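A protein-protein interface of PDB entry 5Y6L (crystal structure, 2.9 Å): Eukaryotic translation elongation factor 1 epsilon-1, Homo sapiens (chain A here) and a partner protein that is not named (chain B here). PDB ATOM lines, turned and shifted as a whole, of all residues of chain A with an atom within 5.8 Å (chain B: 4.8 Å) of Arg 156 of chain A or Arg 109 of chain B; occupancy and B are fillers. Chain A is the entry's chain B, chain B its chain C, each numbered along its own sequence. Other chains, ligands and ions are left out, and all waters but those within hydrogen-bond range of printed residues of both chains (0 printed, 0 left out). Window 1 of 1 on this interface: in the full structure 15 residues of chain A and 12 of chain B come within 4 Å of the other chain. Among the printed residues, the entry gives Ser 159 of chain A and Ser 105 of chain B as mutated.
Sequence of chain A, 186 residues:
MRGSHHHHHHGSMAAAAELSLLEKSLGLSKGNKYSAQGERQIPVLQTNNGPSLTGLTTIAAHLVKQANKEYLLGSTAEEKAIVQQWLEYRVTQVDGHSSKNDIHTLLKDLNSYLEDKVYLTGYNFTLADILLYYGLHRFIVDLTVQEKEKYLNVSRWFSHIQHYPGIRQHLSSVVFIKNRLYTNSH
Of the printed residues of chain B, Arg 156 of chain A touches Arg 109 (3.4 Å), Thr 110 (3.7 Å) and Arg 149 (3.3 Å).
Arg 109 of chain B touches just these residues of chain A: Arg 156 (3.4 Å) and Lys 178 (3.6 Å).
Of the printed residues of chain B, Lys 117 of chain A touches Arg 149 (3.5 Å).
Printed residues of chain B within 4 Å of Leu 152 of chain A: Ser 107 (3.9 Å) and Leu 108 (3.8 Å).
Of the printed residues of chain B, Lys 178 of chain A touches Leu 108 (3.3 Å) and Arg 109 (3.6 Å).
The nearest residue of chain A that does not touch Arg 109 of chain B is Asn 179 of chain A (4.5 Å).
The nearest printed residue of chain A that does not touch Arg 149 of chain B is Asp 116 of chain A (4.3 Å).
CD of Arg 149 of chain B touches O of Glu 115 of chain A (3.6 Å).
Arg 149 of chain B touches Lys 117 of chain A.
CD1 of Leu 152 of chain A touches O of Ser 107 of chain B, 3.9 Å away.
CB of Leu 152 of chain A touches CD2 of Leu 108 of chain B, at 3.8 Å.
Arg 109 of chain B touches Arg 156 of chain A.
Arg 156 of chain A touches Thr 110 of chain B (CG to OG1, 3.7 Å).
His 160 of chain A touches Thr 110 of chain B (CB to OG1, 3.4 Å).
Lys 178 of chain A touches Arg 109 of chain B (O to NH1, 3.6 Å).
Leu 108 of chain B touches Asn 179 of chain A (CD1 to O, 3.6 Å).
O of Leu 108 of chain B sits at hydrogen-bond distance from NZ of Lys 178 of chain A, at 3.3 Å.
The guanidinium group of Arg 156 of chain A sits close to the guanidinium group of Arg 149 of chain B, 3.3 Å away.
Hydrophobic or aromatic side chains of chain B that line the printed part of chain A: Leu 108.
Among the printed residues, no Asp or Glu carboxylate lies within 4 Å of a Lys or Arg side-chain nitrogen of the other chain.
The backbone carbonyl oxygen (O) of Leu 114 of chain A sits at hydrogen-bond distance from the guanidinium group (NH2) of Arg 156 of chain A.
The side-chain amino group of Lys 117 of chain A is in salt-bridge range of the side-chain carboxylate of Asp 116 of chain A (3.1 Å).
The side-chain hydroxyl (OG) of Ser 159 of chain A is in hydrogen-bond range of the side-chain amino group (NZ) of Lys 178 of chain A (2.9 Å).
The backbone carbonyl oxygen of Leu 106 of chain B lies within hydrogen-bond range of the guanidinium group of Arg 149 of chain B, at 2.5 Å.
The backbone carbonyl oxygen of Leu 112 of chain B is in hydrogen-bond range of the guanidinium group of Arg 109 of chain B, at 3.2 Å.
The backbone carbonyl oxygen (O) of Arg 109 of chain B sits at hydrogen-bond distance from the guanidinium group (NH2) of Arg 149 of chain B (3.0 Å).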
ATOM      1  N   LEU A 114     -21.205 -19.216  17.295  1.00  0.00           N
ATOM      2  CA  LEU A 114     -22.111 -19.418  16.176  1.00  0.00           C
ATOM      3  C   LEU A 114     -23.244 -20.397  16.491  1.00  0.00           C
ATOM      4  O   LEU A 114     -24.144 -20.585  15.655  1.00  0.00           O
ATOM      5  CB  LEU A 114     -21.323 -19.901  14.963  1.00  0.00           C
ATOM      6  CG  LEU A 114     -20.536 -18.853  14.191  1.00  0.00           C
ATOM      7  CD1 LEU A 114     -19.790 -19.496  13.040  1.00  0.00           C
ATOM      8  CD2 LEU A 114     -21.473 -17.790  13.680  1.00  0.00           C
ATOM      9  N   GLU A 115     -23.244 -20.992  17.687  1.00  0.00           N
ATOM     10  CA  GLU A 115     -24.144 -22.107  17.953  1.00  0.00           C
ATOM     11  C   GLU A 115     -25.602 -21.722  17.741  1.00  0.00           C
ATOM     12  O   GLU A 115     -26.416 -22.573  17.343  1.00  0.00           O
ATOM     13  CB  GLU A 115     -23.929 -22.629  19.371  1.00  0.00           C
ATOM     14  CG  GLU A 115     -24.822 -23.791  19.730  1.00  0.00           C
ATOM     15  CD  GLU A 115     -24.324 -24.577  20.937  1.00  0.00           C
ATOM     16  OE1 GLU A 115     -24.680 -24.169  22.069  1.00  0.00           O
ATOM     17  OE2 GLU A 115     -23.586 -25.592  20.751  1.00  0.00           O
ATOM     18  N   ASP A 116     -25.938 -20.445  17.970  1.00  0.00           N
ATOM     19  CA  ASP A 116     -27.296 -19.940  17.826  1.00  0.00           C
ATOM     20  C   ASP A 116     -27.438 -18.957  16.681  1.00  0.00           C
ATOM     21  O   ASP A 116     -28.396 -18.175  16.668  1.00  0.00           O
ATOM     22  CB  ASP A 116     -27.774 -19.282  19.120  1.00  0.00           C
ATOM     23  CG  ASP A 116     -26.986 -18.037  19.476  1.00  0.00           C
ATOM     24  OD1 ASP A 116     -25.752 -18.070  19.253  1.00  0.00           O
ATOM     25  OD2 ASP A 116     -27.583 -17.051  20.002  1.00  0.00           O
ATOM     26  N   LYS A 117     -26.510 -18.974  15.719  1.00  0.00           N
ATOM     27  CA  LYS A 117     -26.518 -18.019  14.617  1.00  0.00           C
ATOM     28  C   LYS A 117     -26.350 -18.737  13.283  1.00  0.00           C
ATOM     29  O   LYS A 117     -25.833 -19.858  13.210  1.00  0.00           O
ATOM     30  CB  LYS A 117     -25.416 -16.955  14.783  1.00  0.00           C
ATOM     31  CG  LYS A 117     -25.347 -16.383  16.173  1.00  0.00           C
ATOM     32  CD  LYS A 117     -24.711 -15.032  16.218  1.00  0.00           C
ATOM     33  CE  LYS A 117     -25.004 -14.348  17.555  1.00  0.00           C
ATOM     34  NZ  LYS A 117     -24.673 -15.213  18.729  1.00  0.00           N
ATOM     35  N   VAL A 118     -26.802 -18.076  12.219  1.00  0.00           N
ATOM     36  CA  VAL A 118     -26.488 -18.497  10.864  1.00  0.00           C
ATOM     37  C   VAL A 118     -25.394 -17.635  10.259  1.00  0.00           C
ATOM     38  O   VAL A 118     -24.498 -18.129   9.577  1.00  0.00           O
ATOM     39  CB  VAL A 118     -27.750 -18.475   9.986  1.00  0.00           C
ATOM     40  CG1 VAL A 118     -27.369 -18.714   8.546  1.00  0.00           C
ATOM     41  CG2 VAL A 118     -28.729 -19.538  10.475  1.00  0.00           C
ATOM     42  N   TYR A 151     -15.254 -28.396  15.630  1.00  0.00           N
ATOM     43  CA  TYR A 151     -15.781 -27.065  15.368  1.00  0.00           C
ATOM     44  C   TYR A 151     -16.936 -27.167  14.355  1.00  0.00           C
ATOM     45  O   TYR A 151     -16.901 -26.618  13.245  1.00  0.00           O
ATOM     46  CB  TYR A 151     -14.650 -26.152  14.902  1.00  0.00           C
ATOM     47  CG  TYR A 151     -13.403 -26.294  15.758  1.00  0.00           C
ATOM     48  CD1 TYR A 151     -13.438 -25.965  17.098  1.00  0.00           C
ATOM     49  CD2 TYR A 151     -12.189 -26.779  15.225  1.00  0.00           C
ATOM     50  CE1 TYR A 151     -12.305 -26.111  17.907  1.00  0.00           C
ATOM     51  CE2 TYR A 151     -11.044 -26.916  16.014  1.00  0.00           C
ATOM     52  CZ  TYR A 151     -11.108 -26.581  17.366  1.00  0.00           C
ATOM     53  OH  TYR A 151     -10.023 -26.715  18.223  1.00  0.00           O
ATOM     54  N   LEU A 152     -18.004 -27.878  14.779  1.00  0.00           N
ATOM     55  CA  LEU A 152     -19.083 -28.221  13.845  1.00  0.00           C
ATOM     56  C   LEU A 152     -19.906 -27.008  13.437  1.00  0.00           C
ATOM     57  O   LEU A 152     -20.382 -26.950  12.294  1.00  0.00           O
ATOM     58  CB  LEU A 152     -20.011 -29.295  14.429  1.00  0.00           C
ATOM     59  CG  LEU A 152     -21.155 -28.894  15.355  1.00  0.00           C
ATOM     60  CD1 LEU A 152     -22.009 -30.069  15.695  1.00  0.00           C
ATOM     61  CD2 LEU A 152     -20.597 -28.254  16.609  1.00  0.00           C
ATOM     62  N   ASN A 153     -20.112 -26.043  14.344  1.00  0.00           N
ATOM     63  CA  ASN A 153     -20.842 -24.839  13.954  1.00  0.00           C
ATOM     64  C   ASN A 153     -20.034 -24.018  12.964  1.00  0.00           C
ATOM     65  O   ASN A 153     -20.590 -23.457  12.013  1.00  0.00           O
ATOM     66  CB  ASN A 153     -21.193 -24.000  15.180  1.00  0.00           C
ATOM     67  CG  ASN A 153     -22.138 -24.709  16.110  1.00  0.00           C
ATOM     68  OD1 ASN A 153     -23.041 -25.430  15.668  1.00  0.00           O
ATOM     69  ND2 ASN A 153     -21.946 -24.515  17.406  1.00  0.00           N
ATOM     70  N   VAL A 154     -18.718 -23.938  13.178  1.00  0.00           N
ATOM     71  CA  VAL A 154     -17.863 -23.241  12.232  1.00  0.00           C
ATOM     72  C   VAL A 154     -18.025 -23.851  10.853  1.00  0.00           C
ATOM     73  O   VAL A 154     -18.205 -23.141   9.864  1.00  0.00           O
ATOM     74  CB  VAL A 154     -16.403 -23.272  12.716  1.00  0.00           C
ATOM     75  CG1 VAL A 154     -15.495 -22.629  11.704  1.00  0.00           C
ATOM     76  CG2 VAL A 154     -16.285 -22.508  14.024  1.00  0.00           C
ATOM     77  N   SER A 155     -18.035 -25.181  10.779  1.00  0.00           N
ATOM     78  CA  SER A 155     -18.170 -25.856   9.490  1.00  0.00           C
ATOM     79  C   SER A 155     -19.512 -25.552   8.855  1.00  0.00           C
ATOM     80  O   SER A 155     -19.575 -25.236   7.663  1.00  0.00           O
ATOM     81  CB  SER A 155     -18.012 -27.351   9.674  1.00  0.00           C
ATOM     82  OG  SER A 155     -16.831 -27.646  10.379  1.00  0.00           O
ATOM     83  N   ARG A 156     -20.595 -25.628   9.641  1.00  0.00           N
ATOM     84  CA  ARG A 156     -21.921 -25.307   9.121  1.00  0.00           C
ATOM     85  C   ARG A 156     -21.958 -23.910   8.510  1.00  0.00           C
ATOM     86  O   ARG A 156     -22.397 -23.739   7.364  1.00  0.00           O
ATOM     87  CB  ARG A 156     -22.961 -25.430  10.223  1.00  0.00           C
ATOM     88  CG  ARG A 156     -24.290 -24.849   9.798  1.00  0.00           C
ATOM     89  CD  ARG A 156     -25.302 -24.890  10.906  1.00  0.00           C
ATOM     90  NE  ARG A 156     -24.867 -24.237  12.141  1.00  0.00           N
ATOM     91  CZ  ARG A 156     -24.765 -22.919  12.292  1.00  0.00           C
ATOM     92  NH1 ARG A 156     -25.032 -22.116  11.267  1.00  0.00           N
ATOM     93  NH2 ARG A 156     -24.397 -22.412  13.470  1.00  0.00           N
ATOM     94  N   TRP A 157     -21.502 -22.901   9.273  1.00  0.00           N
ATOM     95  CA  TRP A 157     -21.445 -21.518   8.797  1.00  0.00           C
ATOM     96  C   TRP A 157     -20.554 -21.386   7.557  1.00  0.00           C
ATOM     97  O   TRP A 157     -20.920 -20.718   6.575  1.00  0.00           O
ATOM     98  CB  TRP A 157     -20.942 -20.611   9.928  1.00  0.00           C
ATOM     99  CG  TRP A 157     -20.513 -19.255   9.467  1.00  0.00           C
ATOM    100  CD1 TRP A 157     -21.321 -18.191   9.170  1.00  0.00           C
ATOM    101  CD2 TRP A 157     -19.172 -18.814   9.218  1.00  0.00           C
ATOM    102  NE1 TRP A 157     -20.564 -17.114   8.747  1.00  0.00           N
ATOM    103  CE2 TRP A 157     -19.244 -17.473   8.765  1.00  0.00           C
ATOM    104  CE3 TRP A 157     -17.918 -19.422   9.323  1.00  0.00           C
ATOM    105  CZ2 TRP A 157     -18.105 -16.728   8.431  1.00  0.00           C
ATOM    106  CZ3 TRP A 157     -16.778 -18.675   8.984  1.00  0.00           C
ATOM    107  CH2 TRP A 157     -16.883 -17.342   8.552  1.00  0.00           C
ATOM    108  N   PHE A 158     -19.378 -22.025   7.587  1.00  0.00           N
ATOM    109  CA  PHE A 158     -18.434 -21.960   6.478  1.00  0.00           C
ATOM    110  C   PHE A 158     -19.019 -22.595   5.230  1.00  0.00           C
ATOM    111  O   PHE A 158     -18.984 -22.008   4.140  1.00  0.00           O
ATOM    112  CB  PHE A 158     -17.137 -22.665   6.871  1.00  0.00           C
ATOM    113  CG  PHE A 158     -15.992 -22.344   5.974  1.00  0.00           C
ATOM    114  CD1 PHE A 158     -15.759 -23.093   4.833  1.00  0.00           C
ATOM    115  CD2 PHE A 158     -15.155 -21.271   6.257  1.00  0.00           C
ATOM    116  CE1 PHE A 158     -14.720 -22.782   3.998  1.00  0.00           C
ATOM    117  CE2 PHE A 158     -14.102 -20.960   5.420  1.00  0.00           C
ATOM    118  CZ  PHE A 158     -13.883 -21.717   4.295  1.00  0.00           C
ATOM    119  N   SER A 159     -19.540 -23.815   5.376  1.00  0.00           N
ATOM    120  CA  SER A 159     -20.203 -24.506   4.280  1.00  0.00           C
ATOM    121  C   SER A 159     -21.252 -23.607   3.635  1.00  0.00           C
ATOM    122  O   SER A 159     -21.281 -23.426   2.411  1.00  0.00           O
ATOM    123  CB  SER A 159     -20.844 -25.782   4.817  1.00  0.00           C
ATOM    124  OG  SER A 159     -21.749 -26.323   3.871  1.00  0.00           O
ATOM    125  N   HIS A 160     -22.108 -23.007   4.463  1.00  0.00           N
ATOM    126  CA  HIS A 160     -23.176 -22.177   3.938  1.00  0.00           C
ATOM    127  C   HIS A 160     -22.624 -20.978   3.187  1.00  0.00           C
ATOM    128  O   HIS A 160     -23.097 -20.656   2.094  1.00  0.00           O
ATOM    129  CB  HIS A 160     -24.084 -21.719   5.061  1.00  0.00           C
ATOM    130  CG  HIS A 160     -25.267 -20.961   4.569  1.00  0.00           C
ATOM    131  ND1 HIS A 160     -26.193 -21.512   3.707  1.00  0.00           N
ATOM    132  CD2 HIS A 160     -25.667 -19.687   4.797  1.00  0.00           C
ATOM    133  CE1 HIS A 160     -27.119 -20.608   3.435  1.00  0.00           C
ATOM    134  NE2 HIS A 160     -26.823 -19.494   4.086  1.00  0.00           N
ATOM    135  N   ILE A 161     -21.634 -20.287   3.759  1.00  0.00           N
ATOM    136  CA  ILE A 161     -21.085 -19.117   3.078  1.00  0.00           C
ATOM    137  C   ILE A 161     -20.434 -19.535   1.759  1.00  0.00           C
ATOM    138  O   ILE A 161     -20.701 -18.949   0.705  1.00  0.00           O
ATOM    139  CB  ILE A 161     -20.109 -18.350   3.990  1.00  0.00           C
ATOM    140  CG1 ILE A 161     -20.823 -17.802   5.234  1.00  0.00           C
ATOM    141  CG2 ILE A 161     -19.453 -17.205   3.241  1.00  0.00           C
ATOM    142  CD1 ILE A 161     -21.876 -16.721   4.951  1.00  0.00           C
ATOM    143  N   PHE A 176     -17.382 -30.964   3.169  1.00  0.00           N
ATOM    144  CA  PHE A 176     -17.945 -31.137   4.508  1.00  0.00           C
ATOM    145  C   PHE A 176     -18.878 -32.327   4.498  1.00  0.00           C
ATOM    146  O   PHE A 176     -19.837 -32.351   3.724  1.00  0.00           O
ATOM    147  CB  PHE A 176     -18.716 -29.901   4.974  1.00  0.00           C
ATOM    148  CG  PHE A 176     -17.844 -28.732   5.277  1.00  0.00           C
ATOM    149  CD1 PHE A 176     -17.244 -28.615   6.529  1.00  0.00           C
ATOM    150  CD2 PHE A 176     -17.610 -27.759   4.301  1.00  0.00           C
ATOM    151  CE1 PHE A 176     -16.428 -27.553   6.814  1.00  0.00           C
ATOM    152  CE2 PHE A 176     -16.791 -26.684   4.567  1.00  0.00           C
ATOM    153  CZ  PHE A 176     -16.192 -26.579   5.828  1.00  0.00           C
ATOM    154  N   LYS A 178     -21.942 -34.235   5.871  1.00  0.00           N
ATOM    155  CA  LYS A 178     -23.171 -33.723   6.473  1.00  0.00           C
ATOM    156  C   LYS A 178     -23.759 -34.642   7.548  1.00  0.00           C
ATOM    157  O   LYS A 178     -24.699 -34.239   8.238  1.00  0.00           O
ATOM    158  CB  LYS A 178     -24.233 -33.437   5.388  1.00  0.00           C
ATOM    159  CG  LYS A 178     -23.895 -32.294   4.413  1.00  0.00           C
ATOM    160  CD  LYS A 178     -23.411 -31.072   5.180  1.00  0.00           C
ATOM    161  CE  LYS A 178     -23.176 -29.882   4.260  1.00  0.00           C
ATOM    162  NZ  LYS A 178     -22.975 -28.628   5.046  1.00  0.00           N
ATOM    163  N   ASN A 179     -23.239 -35.845   7.715  1.00  0.00           N
ATOM    164  CA  ASN A 179     -23.625 -36.713   8.815  1.00  0.00           C
ATOM    165  C   ASN A 179     -22.554 -36.660   9.894  1.00  0.00           C
ATOM    166  O   ASN A 179     -21.388 -36.367   9.630  1.00  0.00           O
ATOM    167  CB  ASN A 179     -23.821 -38.152   8.336  1.00  0.00           C
ATOM    168  CG  ASN A 179     -25.140 -38.354   7.621  1.00  0.00           C
ATOM    169  OD1 ASN A 179     -26.205 -37.971   8.120  1.00  0.00           O
ATOM    170  ND2 ASN A 179     -25.084 -38.963   6.449  1.00  0.00           N
ATOM    171  N   GLU B  77     -34.190 -37.175   0.063  1.00  0.00           N
ATOM    172  CA  GLU B  77     -34.124 -36.604   1.399  1.00  0.00           C
ATOM    173  C   GLU B  77     -35.400 -35.845   1.713  1.00  0.00           C
ATOM    174  O   GLU B  77     -35.898 -35.897   2.840  1.00  0.00           O
ATOM    175  CB  GLU B  77     -32.915 -35.675   1.524  1.00  0.00           C
ATOM    176  CG  GLU B  77     -31.542 -36.315   1.401  1.00  0.00           C
ATOM    177  CD  GLU B  77     -30.444 -35.293   1.637  1.00  0.00           C
ATOM    178  OE1 GLU B  77     -29.667 -35.010   0.686  1.00  0.00           O
ATOM    179  OE2 GLU B  77     -30.393 -34.735   2.768  1.00  0.00           O
ATOM    180  N   SER B 105     -29.764 -34.072  13.047  1.00  0.00           N
ATOM    181  CA  SER B 105     -29.608 -33.876  11.611  1.00  0.00           C
ATOM    182  C   SER B 105     -29.119 -32.470  11.305  1.00  0.00           C
ATOM    183  O   SER B 105     -28.210 -32.276  10.484  1.00  0.00           O
ATOM    184  CB  SER B 105     -30.917 -34.134  10.882  1.00  0.00           C
ATOM    185  OG  SER B 105     -31.345 -35.458  11.097  1.00  0.00           O
ATOM    186  N   LEU B 106     -29.721 -31.479  11.953  1.00  0.00           N
ATOM    187  CA  LEU B 106     -29.436 -30.085  11.656  1.00  0.00           C
ATOM    188  C   LEU B 106     -28.132 -29.601  12.255  1.00  0.00           C
ATOM    189  O   LEU B 106     -27.784 -28.428  12.056  1.00  0.00           O
ATOM    190  CB  LEU B 106     -30.579 -29.198  12.153  1.00  0.00           C
ATOM    191  CG  LEU B 106     -31.849 -29.329  11.330  1.00  0.00           C
ATOM    192  CD1 LEU B 106     -33.054 -28.876  12.162  1.00  0.00           C
ATOM    193  CD2 LEU B 106     -31.693 -28.526  10.016  1.00  0.00           C
ATOM    194  N   SER B 107     -27.402 -30.454  12.977  1.00  0.00           N
ATOM    195  CA  SER B 107     -26.174 -29.986  13.605  1.00  0.00           C
ATOM    196  C   SER B 107     -25.125 -29.566  12.567  1.00  0.00           C
ATOM    197  O   SER B 107     -24.283 -28.702  12.855  1.00  0.00           O
ATOM    198  CB  SER B 107     -25.628 -31.052  14.550  1.00  0.00           C
ATOM    199  OG  SER B 107     -25.435 -32.285  13.887  1.00  0.00           O
ATOM    200  N   LEU B 108     -25.184 -30.108  11.347  1.00  0.00           N
ATOM    201  CA  LEU B 108     -24.225 -29.745  10.313  1.00  0.00           C
ATOM    202  C   LEU B 108     -24.857 -29.025   9.137  1.00  0.00           C
ATOM    203  O   LEU B 108     -24.230 -28.916   8.078  1.00  0.00           O
ATOM    204  CB  LEU B 108     -23.499 -30.980   9.805  1.00  0.00           C
ATOM    205  CG  LEU B 108     -22.633 -31.548  10.903  1.00  0.00           C
ATOM    206  CD1 LEU B 108     -22.115 -32.933  10.527  1.00  0.00           C
ATOM    207  CD2 LEU B 108     -21.509 -30.554  11.184  1.00  0.00           C
ATOM    208  N   ARG B 109     -26.083 -28.548   9.280  1.00  0.00           N
ATOM    209  CA  ARG B 109     -26.826 -28.088   8.122  1.00  0.00           C
ATOM    210  C   ARG B 109     -27.510 -26.755   8.410  1.00  0.00           C
ATOM    211  O   ARG B 109     -27.948 -26.483   9.537  1.00  0.00           O
ATOM    212  CB  ARG B 109     -27.862 -29.136   7.700  1.00  0.00           C
ATOM    213  CG  ARG B 109     -27.359 -30.562   7.647  1.00  0.00           C
ATOM    214  CD  ARG B 109     -28.491 -31.529   7.353  1.00  0.00           C
ATOM    215  NE  ARG B 109     -28.447 -31.989   5.969  1.00  0.00           N
ATOM    216  CZ  ARG B 109     -28.147 -33.233   5.609  1.00  0.00           C
ATOM    217  NH1 ARG B 109     -27.870 -34.161   6.529  1.00  0.00           N
ATOM    218  NH2 ARG B 109     -28.142 -33.553   4.323  1.00  0.00           N
ATOM    219  N   THR B 110     -27.599 -25.924   7.374  1.00  0.00           N
ATOM    220  CA  THR B 110     -28.323 -24.676   7.514  1.00  0.00           C
ATOM    221  C   THR B 110     -29.784 -24.854   7.151  1.00  0.00           C
ATOM    222  O   THR B 110     -30.654 -24.379   7.883  1.00  0.00           O
ATOM    223  CB  THR B 110     -27.673 -23.588   6.668  1.00  0.00           C
ATOM    224  OG1 THR B 110     -26.283 -23.515   7.004  1.00  0.00           O
ATOM    225  CG2 THR B 110     -28.335 -22.253   6.944  1.00  0.00           C
ATOM    226  N   TYR B 111     -30.061 -25.535   6.041  1.00  0.00           N
ATOM    227  CA  TYR B 111     -31.385 -26.069   5.733  1.00  0.00           C
ATOM    228  C   TYR B 111     -31.328 -27.594   5.783  1.00  0.00           C
ATOM    229  O   TYR B 111     -30.253 -28.196   5.837  1.00  0.00           O
ATOM    230  CB  TYR B 111     -31.888 -25.598   4.361  1.00  0.00           C
ATOM    231  CG  TYR B 111     -31.985 -24.101   4.200  1.00  0.00           C
ATOM    232  CD1 TYR B 111     -33.107 -23.400   4.628  1.00  0.00           C
ATOM    233  CD2 TYR B 111     -30.952 -23.383   3.604  1.00  0.00           C
ATOM    234  CE1 TYR B 111     -33.180 -22.011   4.479  1.00  0.00           C
ATOM    235  CE2 TYR B 111     -31.014 -21.996   3.449  1.00  0.00           C
ATOM    236  CZ  TYR B 111     -32.122 -21.319   3.882  1.00  0.00           C
ATOM    237  OH  TYR B 111     -32.173 -19.954   3.716  1.00  0.00           O
ATOM    238  N   LEU B 112     -32.504 -28.228   5.768  1.00  0.00           N
ATOM    239  CA  LEU B 112     -32.561 -29.670   5.999  1.00  0.00           C
ATOM    240  C   LEU B 112     -32.018 -30.451   4.816  1.00  0.00           C
ATOM    241  O   LEU B 112     -31.415 -31.515   4.997  1.00  0.00           O
ATOM    242  CB  LEU B 112     -33.991 -30.106   6.298  1.00  0.00           C
ATOM    243  CG  LEU B 112     -34.359 -30.146   7.780  1.00  0.00           C
ATOM    244  CD1 LEU B 112     -35.808 -30.538   7.964  1.00  0.00           C
ATOM    245  CD2 LEU B 112     -33.454 -31.115   8.470  1.00  0.00           C
ATOM    246  N   ARG B 149     -31.903 -23.059  16.690  1.00  0.00           N
ATOM    247  CA  ARG B 149     -31.223 -22.181  15.742  1.00  0.00           C
ATOM    248  C   ARG B 149     -31.931 -22.164  14.390  1.00  0.00           C
ATOM    249  O   ARG B 149     -32.269 -21.096  13.864  1.00  0.00           O
ATOM    250  CB  ARG B 149     -29.767 -22.619  15.574  1.00  0.00           C
ATOM    251  CG  ARG B 149     -29.174 -22.107  14.304  1.00  0.00           C
ATOM    252  CD  ARG B 149     -27.825 -22.668  14.035  1.00  0.00           C
ATOM    253  NE  ARG B 149     -27.726 -24.101  13.739  1.00  0.00           N
ATOM    254  CZ  ARG B 149     -28.206 -24.697  12.653  1.00  0.00           C
ATOM    255  NH1 ARG B 149     -28.900 -24.010  11.749  1.00  0.00           N
ATOM    256  NH2 ARG B 149     -27.991 -25.996  12.472  1.00  0.00           N
